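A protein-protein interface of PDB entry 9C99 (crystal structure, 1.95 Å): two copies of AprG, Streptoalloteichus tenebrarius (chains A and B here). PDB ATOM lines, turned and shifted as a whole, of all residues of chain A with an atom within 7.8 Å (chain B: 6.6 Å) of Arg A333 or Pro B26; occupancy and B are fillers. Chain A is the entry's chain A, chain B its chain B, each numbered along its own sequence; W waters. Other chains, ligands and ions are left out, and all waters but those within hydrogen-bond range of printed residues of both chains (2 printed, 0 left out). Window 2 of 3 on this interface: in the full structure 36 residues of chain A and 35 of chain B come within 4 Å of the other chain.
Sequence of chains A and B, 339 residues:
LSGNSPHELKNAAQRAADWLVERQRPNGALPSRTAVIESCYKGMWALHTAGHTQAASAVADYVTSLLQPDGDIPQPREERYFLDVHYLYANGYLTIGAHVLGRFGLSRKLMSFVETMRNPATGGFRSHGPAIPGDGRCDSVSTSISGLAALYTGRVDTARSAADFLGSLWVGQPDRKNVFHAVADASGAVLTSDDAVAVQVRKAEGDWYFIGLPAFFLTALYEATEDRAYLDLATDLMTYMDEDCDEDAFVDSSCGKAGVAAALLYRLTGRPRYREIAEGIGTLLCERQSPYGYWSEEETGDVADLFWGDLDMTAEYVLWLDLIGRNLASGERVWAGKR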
ATOM      1  N   TYR A 266     -39.357 -14.357  -0.737  1.00  0.00           N
ATOM      2  CA  TYR A 266     -38.480 -13.200  -0.595  1.00  0.00           C
ATOM      3  C   TYR A 266     -37.589 -13.020  -1.819  1.00  0.00           C
ATOM      4  O   TYR A 266     -37.435 -11.900  -2.314  1.00  0.00           O
ATOM      5  CB  TYR A 266     -37.617 -13.315   0.655  1.00  0.00           C
ATOM      6  CG  TYR A 266     -36.630 -12.158   0.760  1.00  0.00           C
ATOM      7  CD1 TYR A 266     -37.089 -10.847   0.904  1.00  0.00           C
ATOM      8  CD2 TYR A 266     -35.265 -12.376   0.723  1.00  0.00           C
ATOM      9  CE1 TYR A 266     -36.201  -9.774   0.990  1.00  0.00           C
ATOM     10  CE2 TYR A 266     -34.354 -11.319   0.817  1.00  0.00           C
ATOM     11  CZ  TYR A 266     -34.837 -10.021   0.947  1.00  0.00           C
ATOM     12  OH  TYR A 266     -33.962  -8.965   1.040  1.00  0.00           O
ATOM     13  N   ARG A 326     -29.903 -20.398   0.634  1.00  0.00           N
ATOM     14  CA  ARG A 326     -29.543 -19.910  -0.691  1.00  0.00           C
ATOM     15  C   ARG A 326     -30.605 -18.984  -1.273  1.00  0.00           C
ATOM     16  O   ARG A 326     -30.268 -18.086  -2.047  1.00  0.00           O
ATOM     17  CB  ARG A 326     -29.241 -21.064  -1.634  1.00  0.00           C
ATOM     18  CG  ARG A 326     -30.404 -21.891  -2.029  1.00  0.00           C
ATOM     19  CD  ARG A 326     -29.909 -23.230  -2.496  1.00  0.00           C
ATOM     20  NE  ARG A 326     -30.759 -23.782  -3.535  1.00  0.00           N
ATOM     21  CZ  ARG A 326     -30.889 -25.078  -3.796  1.00  0.00           C
ATOM     22  NH1 ARG A 326     -31.681 -25.469  -4.791  1.00  0.00           N
ATOM     23  NH2 ARG A 326     -30.246 -25.974  -3.068  1.00  0.00           N
ATOM     24  N   ASN A 327     -31.871 -19.139  -0.893  1.00  0.00           N
ATOM     25  CA  ASN A 327     -32.848 -18.166  -1.353  1.00  0.00           C
ATOM     26  C   ASN A 327     -32.704 -16.844  -0.611  1.00  0.00           C
ATOM     27  O   ASN A 327     -32.896 -15.776  -1.209  1.00  0.00           O
ATOM     28  CB  ASN A 327     -34.256 -18.743  -1.239  1.00  0.00           C
ATOM     29  CG  ASN A 327     -34.522 -19.754  -2.339  1.00  0.00           C
ATOM     30  OD1 ASN A 327     -34.588 -19.383  -3.495  1.00  0.00           O
ATOM     31  ND2 ASN A 327     -34.573 -21.040  -1.992  1.00  0.00           N
ATOM     32  N   LEU A 328     -32.330 -16.884   0.679  1.00  0.00           N
ATOM     33  CA  LEU A 328     -32.067 -15.637   1.394  1.00  0.00           C
ATOM     34  C   LEU A 328     -30.808 -14.964   0.869  1.00  0.00           C
ATOM     35  O   LEU A 328     -30.775 -13.746   0.726  1.00  0.00           O
ATOM     36  CB  LEU A 328     -31.936 -15.876   2.901  1.00  0.00           C
ATOM     37  CG  LEU A 328     -33.253 -16.122   3.636  1.00  0.00           C
ATOM     38  CD1 LEU A 328     -33.046 -16.139   5.148  1.00  0.00           C
ATOM     39  CD2 LEU A 328     -34.314 -15.070   3.248  1.00  0.00           C
ATOM     40  N   ALA A 329     -29.769 -15.738   0.564  1.00  0.00           N
ATOM     41  CA  ALA A 329     -28.541 -15.120   0.066  1.00  0.00           C
ATOM     42  C   ALA A 329     -28.756 -14.494  -1.312  1.00  0.00           C
ATOM     43  O   ALA A 329     -28.287 -13.383  -1.580  1.00  0.00           O
ATOM     44  CB  ALA A 329     -27.407 -16.150   0.033  1.00  0.00           C
ATOM     45  N   SER A 330     -29.457 -15.184  -2.204  1.00  0.00           N
ATOM     46  CA  SER A 330     -29.747 -14.567  -3.502  1.00  0.00           C
ATOM     47  C   SER A 330     -30.769 -13.439  -3.385  1.00  0.00           C
ATOM     48  O   SER A 330     -30.677 -12.443  -4.121  1.00  0.00           O
ATOM     49  CB  SER A 330     -30.222 -15.627  -4.490  1.00  0.00           C
ATOM     50  OG  SER A 330     -29.096 -16.381  -4.929  1.00  0.00           O
ATOM     51  N   GLY A 331     -31.742 -13.577  -2.482  1.00  0.00           N
ATOM     52  CA  GLY A 331     -32.687 -12.489  -2.264  1.00  0.00           C
ATOM     53  C   GLY A 331     -31.992 -11.205  -1.853  1.00  0.00           C
ATOM     54  O   GLY A 331     -32.292 -10.134  -2.374  1.00  0.00           O
ATOM     55  N   GLU A 332     -31.026 -11.302  -0.932  1.00  0.00           N
ATOM     56  CA  GLU A 332     -30.256 -10.129  -0.539  1.00  0.00           C
ATOM     57  C   GLU A 332     -29.525  -9.521  -1.733  1.00  0.00           C
ATOM     58  O   GLU A 332     -29.519  -8.299  -1.912  1.00  0.00           O
ATOM     59  CB  GLU A 332     -29.271 -10.508   0.572  1.00  0.00           C
ATOM     60  CG  GLU A 332     -28.172  -9.472   0.811  1.00  0.00           C
ATOM     61  CD  GLU A 332     -27.922  -9.204   2.284  1.00  0.00           C
ATOM     62  OE1 GLU A 332     -28.907  -9.084   3.050  1.00  0.00           O
ATOM     63  OE2 GLU A 332     -26.741  -9.097   2.668  1.00  0.00           O
ATOM     64  N   ARG A 333     -28.895 -10.367  -2.565  1.00  0.00           N
ATOM     65  CA  ARG A 333     -28.197  -9.863  -3.753  1.00  0.00           C
ATOM     66  C   ARG A 333     -29.156  -9.119  -4.688  1.00  0.00           C
ATOM     67  O   ARG A 333     -28.830  -8.036  -5.183  1.00  0.00           O
ATOM     68  CB  ARG A 333     -27.499 -11.010  -4.499  1.00  0.00           C
ATOM     69  CG  ARG A 333     -26.821 -10.604  -5.841  1.00  0.00           C
ATOM     70  CD  ARG A 333     -26.018 -11.765  -6.486  1.00  0.00           C
ATOM     71  NE  ARG A 333     -24.871 -12.179  -5.674  1.00  0.00           N
ATOM     72  CZ  ARG A 333     -24.876 -13.226  -4.866  1.00  0.00           C
ATOM     73  NH1 ARG A 333     -23.793 -13.515  -4.157  1.00  0.00           N
ATOM     74  NH2 ARG A 333     -25.964 -13.999  -4.761  1.00  0.00           N
ATOM     75  N   VAL A 334     -30.355  -9.667  -4.913  1.00  0.00           N
ATOM     76  CA  VAL A 334     -31.306  -9.067  -5.849  1.00  0.00           C
ATOM     77  C   VAL A 334     -31.944  -7.807  -5.263  1.00  0.00           C
ATOM     78  O   VAL A 334     -32.106  -6.803  -5.963  1.00  0.00           O
ATOM     79  CB  VAL A 334     -32.385 -10.099  -6.251  1.00  0.00           C
ATOM     80  CG1 VAL A 334     -33.529  -9.420  -6.991  1.00  0.00           C
ATOM     81  CG2 VAL A 334     -31.796 -11.185  -7.136  1.00  0.00           C
ATOM     82  N   TRP A 335     -32.320  -7.835  -3.980  1.00  0.00           N
ATOM     83  CA  TRP A 335     -33.213  -6.829  -3.416  1.00  0.00           C
ATOM     84  C   TRP A 335     -32.577  -5.872  -2.411  1.00  0.00           C
ATOM     85  O   TRP A 335     -33.146  -4.808  -2.160  1.00  0.00           O
ATOM     86  CB  TRP A 335     -34.404  -7.515  -2.729  1.00  0.00           C
ATOM     87  CG  TRP A 335     -35.295  -8.273  -3.661  1.00  0.00           C
ATOM     88  CD1 TRP A 335     -35.366  -9.633  -3.812  1.00  0.00           C
ATOM     89  CD2 TRP A 335     -36.247  -7.718  -4.564  1.00  0.00           C
ATOM     90  NE1 TRP A 335     -36.311  -9.950  -4.759  1.00  0.00           N
ATOM     91  CE2 TRP A 335     -36.862  -8.790  -5.237  1.00  0.00           C
ATOM     92  CE3 TRP A 335     -36.644  -6.409  -4.872  1.00  0.00           C
ATOM     93  CZ2 TRP A 335     -37.857  -8.597  -6.199  1.00  0.00           C
ATOM     94  CZ3 TRP A 335     -37.630  -6.223  -5.826  1.00  0.00           C
ATOM     95  CH2 TRP A 335     -38.220  -7.309  -6.489  1.00  0.00           C
ATOM     96  N   ALA A 336     -31.435  -6.204  -1.824  1.00  0.00           N
ATOM     97  CA  ALA A 336     -30.976  -5.427  -0.673  1.00  0.00           C
ATOM     98  C   ALA A 336     -29.892  -4.415  -1.039  1.00  0.00           C
ATOM     99  O   ALA A 336     -29.649  -4.149  -2.221  1.00  0.00           O
ATOM    100  CB  ALA A 336     -30.485  -6.358   0.425  1.00  0.00           C
ATOM    101  N   GLN B  24     -14.915 -16.190  -5.772  1.00  0.00           N
ATOM    102  CA  GLN B  24     -16.111 -15.751  -6.471  1.00  0.00           C
ATOM    103  C   GLN B  24     -16.327 -14.257  -6.260  1.00  0.00           C
ATOM    104  O   GLN B  24     -16.137 -13.737  -5.163  1.00  0.00           O
ATOM    105  CB  GLN B  24     -17.328 -16.531  -5.981  1.00  0.00           C
ATOM    106  CG  GLN B  24     -18.612 -16.245  -6.786  1.00  0.00           C
ATOM    107  CD  GLN B  24     -19.736 -17.207  -6.465  1.00  0.00           C
ATOM    108  OE1 GLN B  24     -19.887 -17.642  -5.323  1.00  0.00           O
ATOM    109  NE2 GLN B  24     -20.504 -17.577  -7.476  1.00  0.00           N
ATOM    110  N   ARG B  25     -16.756 -13.583  -7.309  1.00  0.00           N
ATOM    111  CA  ARG B  25     -16.981 -12.150  -7.254  1.00  0.00           C
ATOM    112  C   ARG B  25     -18.352 -11.829  -6.657  1.00  0.00           C
ATOM    113  O   ARG B  25     -19.223 -12.699  -6.557  1.00  0.00           O
ATOM    114  CB  ARG B  25     -16.825 -11.561  -8.654  1.00  0.00           C
ATOM    115  CG  ARG B  25     -15.357 -11.352  -9.024  1.00  0.00           C
ATOM    116  CD  ARG B  25     -15.072 -11.657 -10.491  1.00  0.00           C
ATOM    117  NE  ARG B  25     -13.640 -11.676 -10.784  1.00  0.00           N
ATOM    118  CZ  ARG B  25     -13.128 -11.811 -12.007  1.00  0.00           C
ATOM    119  NH1 ARG B  25     -13.935 -11.933 -13.058  1.00  0.00           N
ATOM    120  NH2 ARG B  25     -11.811 -11.824 -12.182  1.00  0.00           N
ATOM    121  N   PRO B  26     -18.556 -10.580  -6.202  1.00  0.00           N
ATOM    122  CA  PRO B  26     -19.830 -10.252  -5.533  1.00  0.00           C
ATOM    123  C   PRO B  26     -21.049 -10.422  -6.420  1.00  0.00           C
ATOM    124  O   PRO B  26     -22.114 -10.810  -5.934  1.00  0.00           O
ATOM    125  CB  PRO B  26     -19.647  -8.779  -5.133  1.00  0.00           C
ATOM    126  CG  PRO B  26     -18.198  -8.575  -5.093  1.00  0.00           C
ATOM    127  CD  PRO B  26     -17.615  -9.448  -6.147  1.00  0.00           C
ATOM    128  N   ASN B  27     -20.933 -10.127  -7.712  1.00  0.00           N
ATOM    129  CA  ASN B  27     -22.059 -10.356  -8.604  1.00  0.00           C
ATOM    130  C   ASN B  27     -22.287 -11.841  -8.874  1.00  0.00           C
ATOM    131  O   ASN B  27     -23.261 -12.183  -9.550  1.00  0.00           O
ATOM    132  CB  ASN B  27     -21.855  -9.583  -9.917  1.00  0.00           C
ATOM    133  CG  ASN B  27     -20.710 -10.123 -10.747  1.00  0.00           C
ATOM    134  OD1 ASN B  27     -19.918 -10.942 -10.278  1.00  0.00           O
ATOM    135  ND2 ASN B  27     -20.618  -9.672 -11.995  1.00  0.00           N
ATOM    136  N   GLY B  28     -21.429 -12.728  -8.348  1.00  0.00           N
ATOM    137  CA  GLY B  28     -21.568 -14.153  -8.554  1.00  0.00           C
ATOM    138  C   GLY B  28     -20.694 -14.739  -9.647  1.00  0.00           C
ATOM    139  O   GLY B  28     -20.587 -15.965  -9.736  1.00  0.00           O
ATOM    140  N   ALA B  29     -20.083 -13.910 -10.490  1.00  0.00           N
ATOM    141  CA  ALA B  29     -19.169 -14.415 -11.510  1.00  0.00           C
ATOM    142  C   ALA B  29     -17.982 -15.130 -10.865  1.00  0.00           C
ATOM    143  O   ALA B  29     -17.546 -14.789  -9.767  1.00  0.00           O
ATOM    144  CB  ALA B  29     -18.671 -13.256 -12.384  1.00  0.00           C
ATOM    145  N   GLN B  54     -25.036 -21.879  -2.143  1.00  0.00           N
ATOM    146  CA  GLN B  54     -25.163 -20.427  -2.182  1.00  0.00           C
ATOM    147  C   GLN B  54     -24.276 -19.856  -3.274  1.00  0.00           C
ATOM    148  O   GLN B  54     -24.680 -18.934  -3.993  1.00  0.00           O
ATOM    149  CB  GLN B  54     -24.835 -19.796  -0.822  1.00  0.00           C
ATOM    150  CG  GLN B  54     -26.039 -19.808   0.119  1.00  0.00           C
ATOM    151  CD  GLN B  54     -25.664 -19.623   1.589  1.00  0.00           C
ATOM    152  OE1 GLN B  54     -24.875 -18.747   1.935  1.00  0.00           O
ATOM    153  NE2 GLN B  54     -26.240 -20.448   2.454  1.00  0.00           N
ATOM    154  N   SER B  57     -26.049 -20.633  -6.560  1.00  0.00           N
ATOM    155  CA  SER B  57     -27.151 -19.687  -6.747  1.00  0.00           C
ATOM    156  C   SER B  57     -26.652 -18.313  -7.139  1.00  0.00           C
ATOM    157  O   SER B  57     -27.339 -17.602  -7.872  1.00  0.00           O
ATOM    158  CB  SER B  57     -27.990 -19.539  -5.467  1.00  0.00           C
ATOM    159  OG  SER B  57     -28.625 -20.752  -5.134  1.00  0.00           O
ATOM    160  N   ALA B  58     -25.493 -17.904  -6.628  1.00  0.00           N
ATOM    161  CA  ALA B  58     -24.921 -16.634  -7.054  1.00  0.00           C
ATOM    162  C   ALA B  58     -24.539 -16.663  -8.534  1.00  0.00           C
ATOM    163  O   ALA B  58     -24.744 -15.672  -9.247  1.00  0.00           O
ATOM    164  CB  ALA B  58     -23.714 -16.280  -6.181  1.00  0.00           C
ATOM    165  N   VAL B  59     -23.955 -17.771  -9.013  1.00  0.00           N
ATOM    166  CA  VAL B  59     -23.755 -17.914 -10.460  1.00  0.00           C
ATOM    167  C   VAL B  59     -25.089 -17.819 -11.188  1.00  0.00           C
ATOM    168  O   VAL B  59     -25.194 -17.157 -12.233  1.00  0.00           O
ATOM    169  CB  VAL B  59     -23.028 -19.227 -10.796  1.00  0.00           C
ATOM    170  CG1 VAL B  59     -22.823 -19.345 -12.299  1.00  0.00           C
ATOM    171  CG2 VAL B  59     -21.696 -19.296 -10.055  1.00  0.00           C
ATOM    172  N   ASP B  61     -27.688 -16.162 -10.262  1.00  0.00           N
ATOM    173  CA  ASP B  61     -28.014 -14.739 -10.274  1.00  0.00           C
ATOM    174  C   ASP B  61     -27.275 -14.019 -11.394  1.00  0.00           C
ATOM    175  O   ASP B  61     -27.854 -13.204 -12.123  1.00  0.00           O
ATOM    176  CB  ASP B  61     -27.672 -14.120  -8.920  1.00  0.00           C
ATOM    177  CG  ASP B  61     -28.518 -14.685  -7.788  1.00  0.00           C
ATOM    178  OD1 ASP B  61     -29.609 -15.254  -8.063  1.00  0.00           O
ATOM    179  OD2 ASP B  61     -28.085 -14.552  -6.619  1.00  0.00           O
ATOM    180  N   TYR B  62     -25.981 -14.302 -11.538  1.00  0.00           N
ATOM    181  CA  TYR B  62     -25.180 -13.658 -12.569  1.00  0.00           C
ATOM    182  C   TYR B  62     -25.698 -14.013 -13.955  1.00  0.00           C
ATOM    183  O   TYR B  62     -25.930 -13.132 -14.793  1.00  0.00           O
ATOM    184  CB  TYR B  62     -23.716 -14.061 -12.392  1.00  0.00           C
ATOM    185  CG  TYR B  62     -22.810 -13.609 -13.511  1.00  0.00           C
ATOM    186  CD1 TYR B  62     -22.557 -12.267 -13.721  1.00  0.00           C
ATOM    187  CD2 TYR B  62     -22.207 -14.532 -14.354  1.00  0.00           C
ATOM    188  CE1 TYR B  62     -21.725 -11.851 -14.753  1.00  0.00           C
ATOM    189  CE2 TYR B  62     -21.378 -14.127 -15.381  1.00  0.00           C
ATOM    190  CZ  TYR B  62     -21.142 -12.793 -15.577  1.00  0.00           C
ATOM    191  OH  TYR B  62     -20.303 -12.408 -16.606  1.00  0.00           O
ATOM    192  N   ARG B 103     -34.116 -23.483 -10.127  1.00  0.00           N
ATOM    193  CA  ARG B 103     -34.400 -22.215 -10.803  1.00  0.00           C
ATOM    194  C   ARG B 103     -35.158 -22.543 -12.086  1.00  0.00           C
ATOM    195  O   ARG B 103     -34.629 -22.489 -13.196  1.00  0.00           O
ATOM    196  CB  ARG B 103     -33.120 -21.449 -11.098  1.00  0.00           C
ATOM    197  CG  ARG B 103     -32.369 -21.013  -9.868  1.00  0.00           C
ATOM    198  CD  ARG B 103     -32.959 -19.743  -9.298  1.00  0.00           C
ATOM    199  NE  ARG B 103     -32.126 -19.239  -8.210  1.00  0.00           N
ATOM    200  CZ  ARG B 103     -31.413 -18.120  -8.276  1.00  0.00           C
ATOM    201  NH1 ARG B 103     -31.438 -17.380  -9.379  1.00  0.00           N
ATOM    202  NH2 ARG B 103     -30.688 -17.739  -7.232  1.00  0.00           N
HETATM  203  O   HOH W   1     -27.531 -22.859   1.345  1.00  0.00           O
HETATM  204  O   HOH W   2     -26.479 -16.857  -3.345  1.00  0.00           O
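The backbone carbonyl oxygen (O) of Ser B57 is in hydrogen-bond range of the guanidinium group (NH2) of Arg B103 (3.4 Å).
The side-chain carboxylate of Asp B61 is in salt-bridge range of the guanidinium group of Arg B103.
Water W2 lies within hydrogen-bond range of the backbone carbonyl oxygen (O) of Gln B54, the side-chain hydroxyl (OG) of Ser A330 and the guanidinium group (NH2) of Arg A333.
Water W1 lies within hydrogen-bond range of NE2 of Gln B54 (3.0 Å) and N of Arg A326 (3.5 Å).
Of the 13 printed residues of chain B, 6 touch a printed residue of chain A.
Printed residues of chain B that touch a printed residue of chain A: Pro B26, Gln B54, Ser B57, Ala B58, Asp B61 and Arg B103.
Hydrophobic or aromatic side chains of chain B within 4 Å of the printed part of chain A: Ala B58.
Of the 12 printed residues of chain A, 4 touch a printed residue of chain B.
Hydrophobic or aromatic side chains of chain A that line the printed part of chain B: Ala A329.
Along chain A the printed residues that touch a printed residue of chain B span positions 326 to 333.
Among the printed residues, 9 pairs touch across the chains.
Among the printed residues, Asp or Glu carboxylates within 4 Å of a Lys or Arg side-chain nitrogen of the other chain: Arg A333 with Asp B61 (2.9 Å).
Among the printed residues, pairs that only touch across the chains: Ser A330 with Ser B57 (3.4 Å), Arg A333 with Ala B58 (3.4 Å), Arg A326 with Ser B57 (3.6 Å), Arg A326 with Gln B54 (3.6 Å) and Ala A329 with Gln B54 (3.9 Å).
Of the printed residues of chain B, Arg A326 touches Gln B54 and Ser B57.
Of the printed residues of chain B, Ser A330 touches Ser B57, Asp B61 and Arg B103.
Of the printed residues of chain B, Arg A333 touches Pro B26, Ala B58 and Asp B61.
Of chain A, only Arg A333 (3.1 Å) comes within 4 Å of Pro B26.
Of the printed residues of chain A, Gln B54 touches Arg A326 (3.6 Å) and Ala A329 (3.9 Å).
Of the printed residues of chain A, Ser B57 touches Arg A326 and Ser A330.
Printed residues of chain A within 4 Å of Ala B58: Arg A333.
No position is printed for both chains.
The side-chain carboxylate (OD2) of Asp B61 is in hydrogen-bond range of the side-chain hydroxyl (OG) of Ser A330 (2.7 Å).
NH2 of Arg A333 is in salt-bridge range of OD2 of Asp B61, 2.9 Å away.
The side-chain hydroxyl (OG) of Ser A330 lies within hydrogen-bond range of the guanidinium group (NH2) of Arg B103 (3.1 Å).
The backbone carbonyl oxygen of Pro B26 is in hydrogen-bond range of the guanidinium group of Arg A333 (3.1 Å).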
